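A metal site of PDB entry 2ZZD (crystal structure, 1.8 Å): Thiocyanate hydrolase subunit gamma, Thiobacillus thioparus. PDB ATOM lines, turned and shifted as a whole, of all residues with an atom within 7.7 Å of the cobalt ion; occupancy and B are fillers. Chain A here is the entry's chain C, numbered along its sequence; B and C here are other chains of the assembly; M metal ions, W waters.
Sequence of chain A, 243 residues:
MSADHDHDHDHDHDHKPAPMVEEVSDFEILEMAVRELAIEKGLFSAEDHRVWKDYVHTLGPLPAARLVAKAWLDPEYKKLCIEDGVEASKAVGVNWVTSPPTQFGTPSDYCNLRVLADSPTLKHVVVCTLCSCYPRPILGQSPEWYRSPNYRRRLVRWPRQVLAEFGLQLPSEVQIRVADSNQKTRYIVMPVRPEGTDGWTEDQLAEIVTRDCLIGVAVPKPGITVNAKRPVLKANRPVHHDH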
ATOM      1  N   SER A 108      -6.584  14.560  18.735  1.00  0.00           N
ATOM      2  CA  SER A 108      -5.437  15.306  19.234  1.00  0.00           C
ATOM      3  C   SER A 108      -4.063  15.050  18.630  1.00  0.00           C
ATOM      4  O   SER A 108      -3.180  15.903  18.750  1.00  0.00           O
ATOM      5  CB  SER A 108      -5.356  15.128  20.763  1.00  0.00           C
ATOM      6  OG  SER A 108      -6.531  15.622  21.376  1.00  0.00           O
ATOM      7  N   VAL A 127      10.122  17.958  21.510  1.00  0.00           N
ATOM      8  CA  VAL A 127       9.382  18.567  22.615  1.00  0.00           C
ATOM      9  C   VAL A 127       8.161  19.293  22.040  1.00  0.00           C
ATOM     10  O   VAL A 127       8.071  19.520  20.830  1.00  0.00           O
ATOM     11  CB  VAL A 127      10.252  19.609  23.384  1.00  0.00           C
ATOM     12  CG1 VAL A 127      10.646  20.763  22.468  1.00  0.00           C
ATOM     13  CG2 VAL A 127       9.497  20.144  24.601  1.00  0.00           C
ATOM     14  N   CYS A 128       7.210  19.609  22.905  1.00  0.00           N
ATOM     15  CA  CYS A 128       6.036  20.386  22.513  1.00  0.00           C
ATOM     16  C   CYS A 128       6.062  21.485  23.567  1.00  0.00           C
ATOM     17  O   CYS A 128       5.540  21.308  24.656  1.00  0.00           O
ATOM     18  CB  CYS A 128       4.737  19.591  22.661  1.00  0.00           C
ATOM     19  SG  CYS A 128       3.257  20.629  22.378  1.00  0.00           S
ATOM     20  N   THR A 129       6.687  22.623  23.246  1.00  0.00           N
ATOM     21  CA  THR A 129       6.780  23.678  24.237  1.00  0.00           C
ATOM     22  C   THR A 129       5.428  24.221  24.656  1.00  0.00           C
ATOM     23  O   THR A 129       5.274  24.671  25.785  1.00  0.00           O
ATOM     24  CB  THR A 129       7.667  24.858  23.755  1.00  0.00           C
ATOM     25  OG1 THR A 129       7.091  25.459  22.578  1.00  0.00           O
ATOM     26  CG2 THR A 129       9.075  24.375  23.440  1.00  0.00           C
ATOM     27  N   LEU A 130       4.437  24.153  23.772  1.00  0.00           N
ATOM     28  CA  LEU A 130       3.117  24.664  24.084  1.00  0.00           C
ATOM     29  C   LEU A 130       2.287  23.726  24.945  1.00  0.00           C
ATOM     30  O   LEU A 130       1.336  24.163  25.596  1.00  0.00           O
ATOM     31  CB  LEU A 130       2.360  24.979  22.784  1.00  0.00           C
ATOM     32  CG  LEU A 130       3.027  26.054  21.925  1.00  0.00           C
ATOM     33  CD1 LEU A 130       2.188  26.299  20.674  1.00  0.00           C
ATOM     34  CD2 LEU A 130       3.186  27.340  22.721  1.00  0.00           C
ATOM     35  N   CSD A 131       2.646  22.451  24.958  1.00  0.00           N
ATOM     36  CA  CSD A 131       1.915  21.472  25.754  1.00  0.00           C
ATOM     37  CB  CSD A 131       0.425  21.393  25.415  1.00  0.00           C
ATOM     38  SG  CSD A 131       0.133  21.058  23.639  1.00  0.00           S
ATOM     39  C   CSD A 131       2.529  20.098  25.997  1.00  0.00           C
ATOM     40  O   CSD A 131       3.292  19.910  26.940  1.00  0.00           O
ATOM     41  OD1 CSD A 131       0.379  22.252  22.888  1.00  0.00           O
ATOM     42  OD2 CSD A 131      -1.290  20.634  23.455  1.00  0.00           O
ATOM     43  N   SER A 132       2.197  19.138  25.152  1.00  0.00           N
ATOM     44  CA  SER A 132       2.728  17.792  25.323  1.00  0.00           C
ATOM     45  C   SER A 132       2.551  16.955  24.071  1.00  0.00           C
ATOM     46  O   SER A 132       2.659  15.731  24.093  1.00  0.00           O
ATOM     47  CB  SER A 132       2.051  17.103  26.501  1.00  0.00           C
ATOM     48  OG  SER A 132       0.639  17.100  26.350  1.00  0.00           O
ATOM     49  N   CSD A 133       2.251  17.636  22.976  1.00  0.00           N
ATOM     50  CA  CSD A 133       2.081  16.980  21.699  1.00  0.00           C
ATOM     51  CB  CSD A 133       1.856  17.963  20.576  1.00  0.00           C
ATOM     52  SG  CSD A 133       0.622  19.197  21.123  1.00  0.00           S
ATOM     53  C   CSD A 133       3.065  15.846  21.457  1.00  0.00           C
ATOM     54  O   CSD A 133       4.282  16.046  21.518  1.00  0.00           O
ATOM     55  OD1 CSD A 133      -0.656  18.559  21.242  1.00  0.00           O
ATOM     56  OD2 CSD A 133       0.538  20.345  20.171  1.00  0.00           O
ATOM     57  N   TYR A 134       2.524  14.666  21.198  1.00  0.00           N
ATOM     58  CA  TYR A 134       3.310  13.456  21.100  1.00  0.00           C
ATOM     59  C   TYR A 134       2.673  12.510  20.083  1.00  0.00           C
ATOM     60  O   TYR A 134       1.454  12.495  19.926  1.00  0.00           O
ATOM     61  CB  TYR A 134       3.279  12.876  22.512  1.00  0.00           C
ATOM     62  CG  TYR A 134       4.244  11.777  22.876  1.00  0.00           C
ATOM     63  CD1 TYR A 134       5.535  12.072  23.312  1.00  0.00           C
ATOM     64  CD2 TYR A 134       3.817  10.455  22.921  1.00  0.00           C
ATOM     65  CE1 TYR A 134       6.368  11.077  23.800  1.00  0.00           C
ATOM     66  CE2 TYR A 134       4.645   9.449  23.402  1.00  0.00           C
ATOM     67  CZ  TYR A 134       5.910   9.770  23.851  1.00  0.00           C
ATOM     68  OH  TYR A 134       6.719   8.782  24.365  1.00  0.00           O
ATOM     69  N   ARG A 136       1.264   9.733  19.784  1.00  0.00           N
ATOM     70  CA  ARG A 136       0.603   8.643  20.491  1.00  0.00           C
ATOM     71  C   ARG A 136       0.232   7.382  19.696  1.00  0.00           C
ATOM     72  O   ARG A 136       0.461   6.264  20.166  1.00  0.00           O
ATOM     73  CB  ARG A 136      -0.660   9.163  21.196  1.00  0.00           C
ATOM     74  CG  ARG A 136      -0.407  10.253  22.254  1.00  0.00           C
ATOM     75  CD  ARG A 136      -1.695  10.493  23.038  1.00  0.00           C
ATOM     76  NE  ARG A 136      -1.612  11.548  24.052  1.00  0.00           N
ATOM     77  CZ  ARG A 136      -1.940  12.819  23.848  1.00  0.00           C
ATOM     78  NH1 ARG A 136      -2.364  13.220  22.659  1.00  0.00           N
ATOM     79  NH2 ARG A 136      -1.861  13.683  24.858  1.00  0.00           N
ATOM     80  N   TYR A 146       8.060  14.806  30.064  1.00  0.00           N
ATOM     81  CA  TYR A 146       7.902  15.404  28.743  1.00  0.00           C
ATOM     82  C   TYR A 146       6.836  16.508  28.801  1.00  0.00           C
ATOM     83  O   TYR A 146       6.902  17.498  28.061  1.00  0.00           O
ATOM     84  CB  TYR A 146       7.499  14.320  27.735  1.00  0.00           C
ATOM     85  CG  TYR A 146       7.364  14.783  26.303  1.00  0.00           C
ATOM     86  CD1 TYR A 146       8.461  14.814  25.440  1.00  0.00           C
ATOM     87  CD2 TYR A 146       6.120  15.166  25.789  1.00  0.00           C
ATOM     88  CE1 TYR A 146       8.326  15.214  24.104  1.00  0.00           C
ATOM     89  CE2 TYR A 146       5.971  15.572  24.469  1.00  0.00           C
ATOM     90  CZ  TYR A 146       7.070  15.585  23.634  1.00  0.00           C
ATOM     91  OH  TYR A 146       6.924  15.990  22.328  1.00  0.00           O
ATOM     92  N   ARG A 152       9.720  21.776  28.836  1.00  0.00           N
ATOM     93  CA  ARG A 152       9.170  22.634  27.800  1.00  0.00           C
ATOM     94  C   ARG A 152       9.827  24.017  27.734  1.00  0.00           C
ATOM     95  O   ARG A 152       9.879  24.641  26.680  1.00  0.00           O
ATOM     96  CB  ARG A 152       7.655  22.745  27.992  1.00  0.00           C
ATOM     97  CG  ARG A 152       6.949  21.402  27.809  1.00  0.00           C
ATOM     98  CD  ARG A 152       5.506  21.480  28.290  1.00  0.00           C
ATOM     99  NE  ARG A 152       4.892  22.720  27.837  1.00  0.00           N
ATOM    100  CZ  ARG A 152       4.035  23.423  28.556  1.00  0.00           C
ATOM    101  NH1 ARG A 152       3.670  23.017  29.760  1.00  0.00           N
ATOM    102  NH2 ARG A 152       3.564  24.575  28.086  1.00  0.00           N
ATOM    103  N   ASP A 180      10.208  21.302  17.713  1.00  0.00           N
ATOM    104  CA  ASP A 180       9.104  21.736  18.571  1.00  0.00           C
ATOM    105  C   ASP A 180       7.799  21.416  17.841  1.00  0.00           C
ATOM    106  O   ASP A 180       7.452  22.056  16.849  1.00  0.00           O
ATOM    107  CB  ASP A 180       9.208  23.245  18.845  1.00  0.00           C
ATOM    108  CG  ASP A 180       8.287  23.707  19.958  1.00  0.00           C
ATOM    109  OD1 ASP A 180       7.419  22.922  20.405  1.00  0.00           O
ATOM    110  OD2 ASP A 180       8.420  24.875  20.386  1.00  0.00           O
ATOM    111  N   SER A 181       7.080  20.411  18.354  1.00  0.00           N
ATOM    112  CA  SER A 181       5.814  19.934  17.789  1.00  0.00           C
ATOM    113  C   SER A 181       4.666  20.873  18.155  1.00  0.00           C
ATOM    114  O   SER A 181       3.811  20.521  18.957  1.00  0.00           O
ATOM    115  CB  SER A 181       5.500  18.541  18.329  1.00  0.00           C
ATOM    116  OG  SER A 181       6.675  17.760  18.470  1.00  0.00           O
ATOM    117  N   ASN A 182       4.632  22.051  17.541  1.00  0.00           N
ATOM    118  CA  ASN A 182       3.610  23.045  17.857  1.00  0.00           C
ATOM    119  C   ASN A 182       2.346  23.070  17.008  1.00  0.00           C
ATOM    120  O   ASN A 182       1.368  23.708  17.404  1.00  0.00           O
ATOM    121  CB  ASN A 182       4.257  24.433  17.836  1.00  0.00           C
ATOM    122  CG  ASN A 182       4.725  24.809  16.445  1.00  0.00           C
ATOM    123  OD1 ASN A 182       5.158  23.968  15.674  1.00  0.00           O
ATOM    124  ND2 ASN A 182       4.648  26.110  16.123  1.00  0.00           N
ATOM    125  N   GLN A 183       2.340  22.415  15.859  1.00  0.00           N
ATOM    126  CA  GLN A 183       1.135  22.422  15.030  1.00  0.00           C
ATOM    127  C   GLN A 183       0.593  21.005  14.878  1.00  0.00           C
ATOM    128  O   GLN A 183       0.509  20.266  15.865  1.00  0.00           O
ATOM    129  CB  GLN A 183       1.428  23.080  13.673  1.00  0.00           C
ATOM    130  CG  GLN A 183       2.092  24.478  13.765  1.00  0.00           C
ATOM    131  CD  GLN A 183       1.171  25.592  14.283  1.00  0.00           C
ATOM    132  OE1 GLN A 183      -0.038  25.398  14.449  1.00  0.00           O
ATOM    133  NE2 GLN A 183       1.750  26.764  14.521  1.00  0.00           N
ATOM    134  N   ARG A 186       3.576  15.427  14.210  1.00  0.00           N
ATOM    135  CA  ARG A 186       4.105  14.727  15.381  1.00  0.00           C
ATOM    136  C   ARG A 186       5.381  14.057  14.850  1.00  0.00           C
ATOM    137  O   ARG A 186       5.437  13.688  13.682  1.00  0.00           O
ATOM    138  CB  ARG A 186       3.128  13.664  15.890  1.00  0.00           C
ATOM    139  CG  ARG A 186       1.810  14.245  16.406  1.00  0.00           C
ATOM    140  CD  ARG A 186       2.006  15.146  17.631  1.00  0.00           C
ATOM    141  NE  ARG A 186       0.744  15.769  18.021  1.00  0.00           N
ATOM    142  CZ  ARG A 186       0.323  16.961  17.589  1.00  0.00           C
ATOM    143  NH1 ARG A 186       1.074  17.684  16.768  1.00  0.00           N
ATOM    144  NH2 ARG A 186      -0.867  17.422  17.967  1.00  0.00           N
ATOM    145  N   ARG B  55      -0.101  29.933  18.278  1.00  0.00           N
ATOM    146  CA  ARG B  55       0.691  28.725  18.358  1.00  0.00           C
ATOM    147  C   ARG B  55       2.037  28.996  17.685  1.00  0.00           C
ATOM    148  O   ARG B  55       2.763  28.079  17.306  1.00  0.00           O
ATOM    149  CB  ARG B  55      -0.018  27.528  17.714  1.00  0.00           C
ATOM    150  CG  ARG B  55      -1.230  27.051  18.528  1.00  0.00           C
ATOM    151  CD  ARG B  55      -1.659  25.641  18.139  1.00  0.00           C
ATOM    152  NE  ARG B  55      -0.762  24.604  18.666  1.00  0.00           N
ATOM    153  CZ  ARG B  55      -0.755  24.213  19.942  1.00  0.00           C
ATOM    154  NH1 ARG B  55      -1.581  24.754  20.825  1.00  0.00           N
ATOM    155  NH2 ARG B  55       0.108  23.272  20.337  1.00  0.00           N
ATOM    156  N   ARG C  90      -9.968  22.635  22.369  1.00  0.00           N
ATOM    157  CA  ARG C  90      -9.605  22.145  23.704  1.00  0.00           C
ATOM    158  C   ARG C  90      -8.309  22.797  24.205  1.00  0.00           C
ATOM    159  O   ARG C  90      -8.262  23.298  25.325  1.00  0.00           O
ATOM    160  CB  ARG C  90      -9.429  20.625  23.719  1.00  0.00           C
ATOM    161  CG  ARG C  90      -8.947  20.094  25.071  1.00  0.00           C
ATOM    162  CD  ARG C  90      -8.843  18.579  25.097  1.00  0.00           C
ATOM    163  NE  ARG C  90      -7.903  18.063  24.092  1.00  0.00           N
ATOM    164  CZ  ARG C  90      -6.593  18.238  24.125  1.00  0.00           C
ATOM    165  NH1 ARG C  90      -6.020  18.913  25.113  1.00  0.00           N
ATOM    166  NH2 ARG C  90      -5.833  17.737  23.153  1.00  0.00           N
ATOM    167  N   ARG C  91      -7.273  22.797  23.371  1.00  0.00           N
ATOM    168  CA  ARG C  91      -5.980  23.379  23.768  1.00  0.00           C
ATOM    169  C   ARG C  91      -6.121  24.833  24.194  1.00  0.00           C
ATOM    170  O   ARG C  91      -5.593  25.254  25.221  1.00  0.00           O
ATOM    171  CB  ARG C  91      -4.961  23.298  22.630  1.00  0.00           C
ATOM    172  CG  ARG C  91      -4.523  21.874  22.330  1.00  0.00           C
ATOM    173  CD  ARG C  91      -3.307  21.811  21.395  1.00  0.00           C
ATOM    174  NE  ARG C  91      -3.033  20.422  21.055  1.00  0.00           N
ATOM    175  CZ  ARG C  91      -3.622  19.772  20.057  1.00  0.00           C
ATOM    176  NH1 ARG C  91      -4.498  20.396  19.287  1.00  0.00           N
ATOM    177  NH2 ARG C  91      -3.351  18.491  19.867  1.00  0.00           N
ATOM    178  N   ASN C  95      -5.120  25.085  27.928  1.00  0.00           N
ATOM    179  CA  ASN C  95      -3.764  25.570  28.160  1.00  0.00           C
ATOM    180  C   ASN C  95      -3.604  27.076  28.163  1.00  0.00           C
ATOM    181  O   ASN C  95      -2.528  27.577  28.484  1.00  0.00           O
ATOM    182  CB  ASN C  95      -2.826  24.952  27.114  1.00  0.00           C
ATOM    183  CG  ASN C  95      -2.978  23.456  27.018  1.00  0.00           C
ATOM    184  OD1 ASN C  95      -3.180  22.784  28.032  1.00  0.00           O
ATOM    185  ND2 ASN C  95      -2.864  22.903  25.809  1.00  0.00           N
ATOM    186  N   TYR C 108      -1.500  18.840  35.404  1.00  0.00           N
ATOM    187  CA  TYR C 108      -1.699  18.682  33.977  1.00  0.00           C
ATOM    188  C   TYR C 108      -3.115  18.147  33.671  1.00  0.00           C
ATOM    189  O   TYR C 108      -3.919  18.828  33.023  1.00  0.00           O
ATOM    190  CB  TYR C 108      -0.632  17.717  33.463  1.00  0.00           C
ATOM    191  CG  TYR C 108      -0.734  17.236  32.030  1.00  0.00           C
ATOM    192  CD1 TYR C 108      -0.135  17.943  30.993  1.00  0.00           C
ATOM    193  CD2 TYR C 108      -1.349  16.019  31.736  1.00  0.00           C
ATOM    194  CE1 TYR C 108      -0.123  17.428  29.685  1.00  0.00           C
ATOM    195  CE2 TYR C 108      -1.347  15.504  30.452  1.00  0.00           C
ATOM    196  CZ  TYR C 108      -0.730  16.202  29.426  1.00  0.00           C
ATOM    197  OH  TYR C 108      -0.690  15.666  28.156  1.00  0.00           O
ATOM    198  N   TRP C 112      -7.044  19.346  32.094  1.00  0.00           N
ATOM    199  CA  TRP C 112      -7.769  18.624  31.053  1.00  0.00           C
ATOM    200  C   TRP C 112      -9.204  18.388  31.519  1.00  0.00           C
ATOM    201  O   TRP C 112     -10.150  18.623  30.776  1.00  0.00           O
ATOM    202  CB  TRP C 112      -7.150  17.252  30.774  1.00  0.00           C
ATOM    203  CG  TRP C 112      -5.945  17.230  29.858  1.00  0.00           C
ATOM    204  CD1 TRP C 112      -4.694  17.706  30.140  1.00  0.00           C
ATOM    205  CD2 TRP C 112      -5.876  16.640  28.560  1.00  0.00           C
ATOM    206  NE1 TRP C 112      -3.844  17.432  29.084  1.00  0.00           N
ATOM    207  CE2 TRP C 112      -4.538  16.786  28.101  1.00  0.00           C
ATOM    208  CE3 TRP C 112      -6.805  16.001  27.723  1.00  0.00           C
ATOM    209  CZ2 TRP C 112      -4.123  16.307  26.848  1.00  0.00           C
ATOM    210  CZ3 TRP C 112      -6.383  15.533  26.478  1.00  0.00           C
ATOM    211  CH2 TRP C 112      -5.045  15.682  26.055  1.00  0.00           C
HETATM  212 CO    CO M   1       1.430  19.378  23.191  1.00  0.00          CO
HETATM  213  O   HOH W   1      -0.242  18.281  23.893  1.00  0.00           O
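Four residues have an atom within 4 Å of the cobalt ion: Cys 128, CSD 131, Ser 132 and CSD 133.
The guanidinium group (NH2) of Arg 55 of chain B lies within salt-bridge range of OD1 of CSD 131, 2.8 Å away. OD2 of CSD 131 is in salt-bridge range of NE of Arg 91 of chain C, at 3.0 Å. The side-chain hydroxyl (OG) of Ser 132 lies within hydrogen-bond range of the side-chain hydroxyl (OH) of Tyr 108 of chain C, 2.7 Å away. SG of Cys 128 lies close to O of Ser 181, at 3.5 Å. The guanidinium group (NH2) of Arg 91 of chain C lies within salt-bridge range of OD1 of CSD 133 (3.0 Å). O of CSD 133 sits at hydrogen-bond distance from OH of Tyr 146 (2.8 Å). OD1 of CSD 133 lies within salt-bridge range of the guanidinium group (NH2) of Arg 186 (3.5 Å). OD2 of CSD 133 lies within salt-bridge range of the guanidinium group (NH2) of Arg 55 of chain B, at 3.0 Å.
Water W1 lies within hydrogen-bond range of OD2 of CSD 131 (2.6 Å), OD1 of CSD 133 (2.7 Å) and the side-chain hydroxyl of Ser 132 (2.9 Å).
N of CSD 133 is bound to the cobalt ion. The cobalt ion is bound by the backbone nitrogen (N) of Ser 132. Water W1 is bound to the cobalt ion (2.1 Å). The cobalt ion is bound by SG of CSD 131 (2.2 Å). SG of CSD 133 is bound to the cobalt ion, at 2.2 Å. SG of Cys 128 is bound to the cobalt ion. The cobalt ion has six donor atoms within binding distance.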
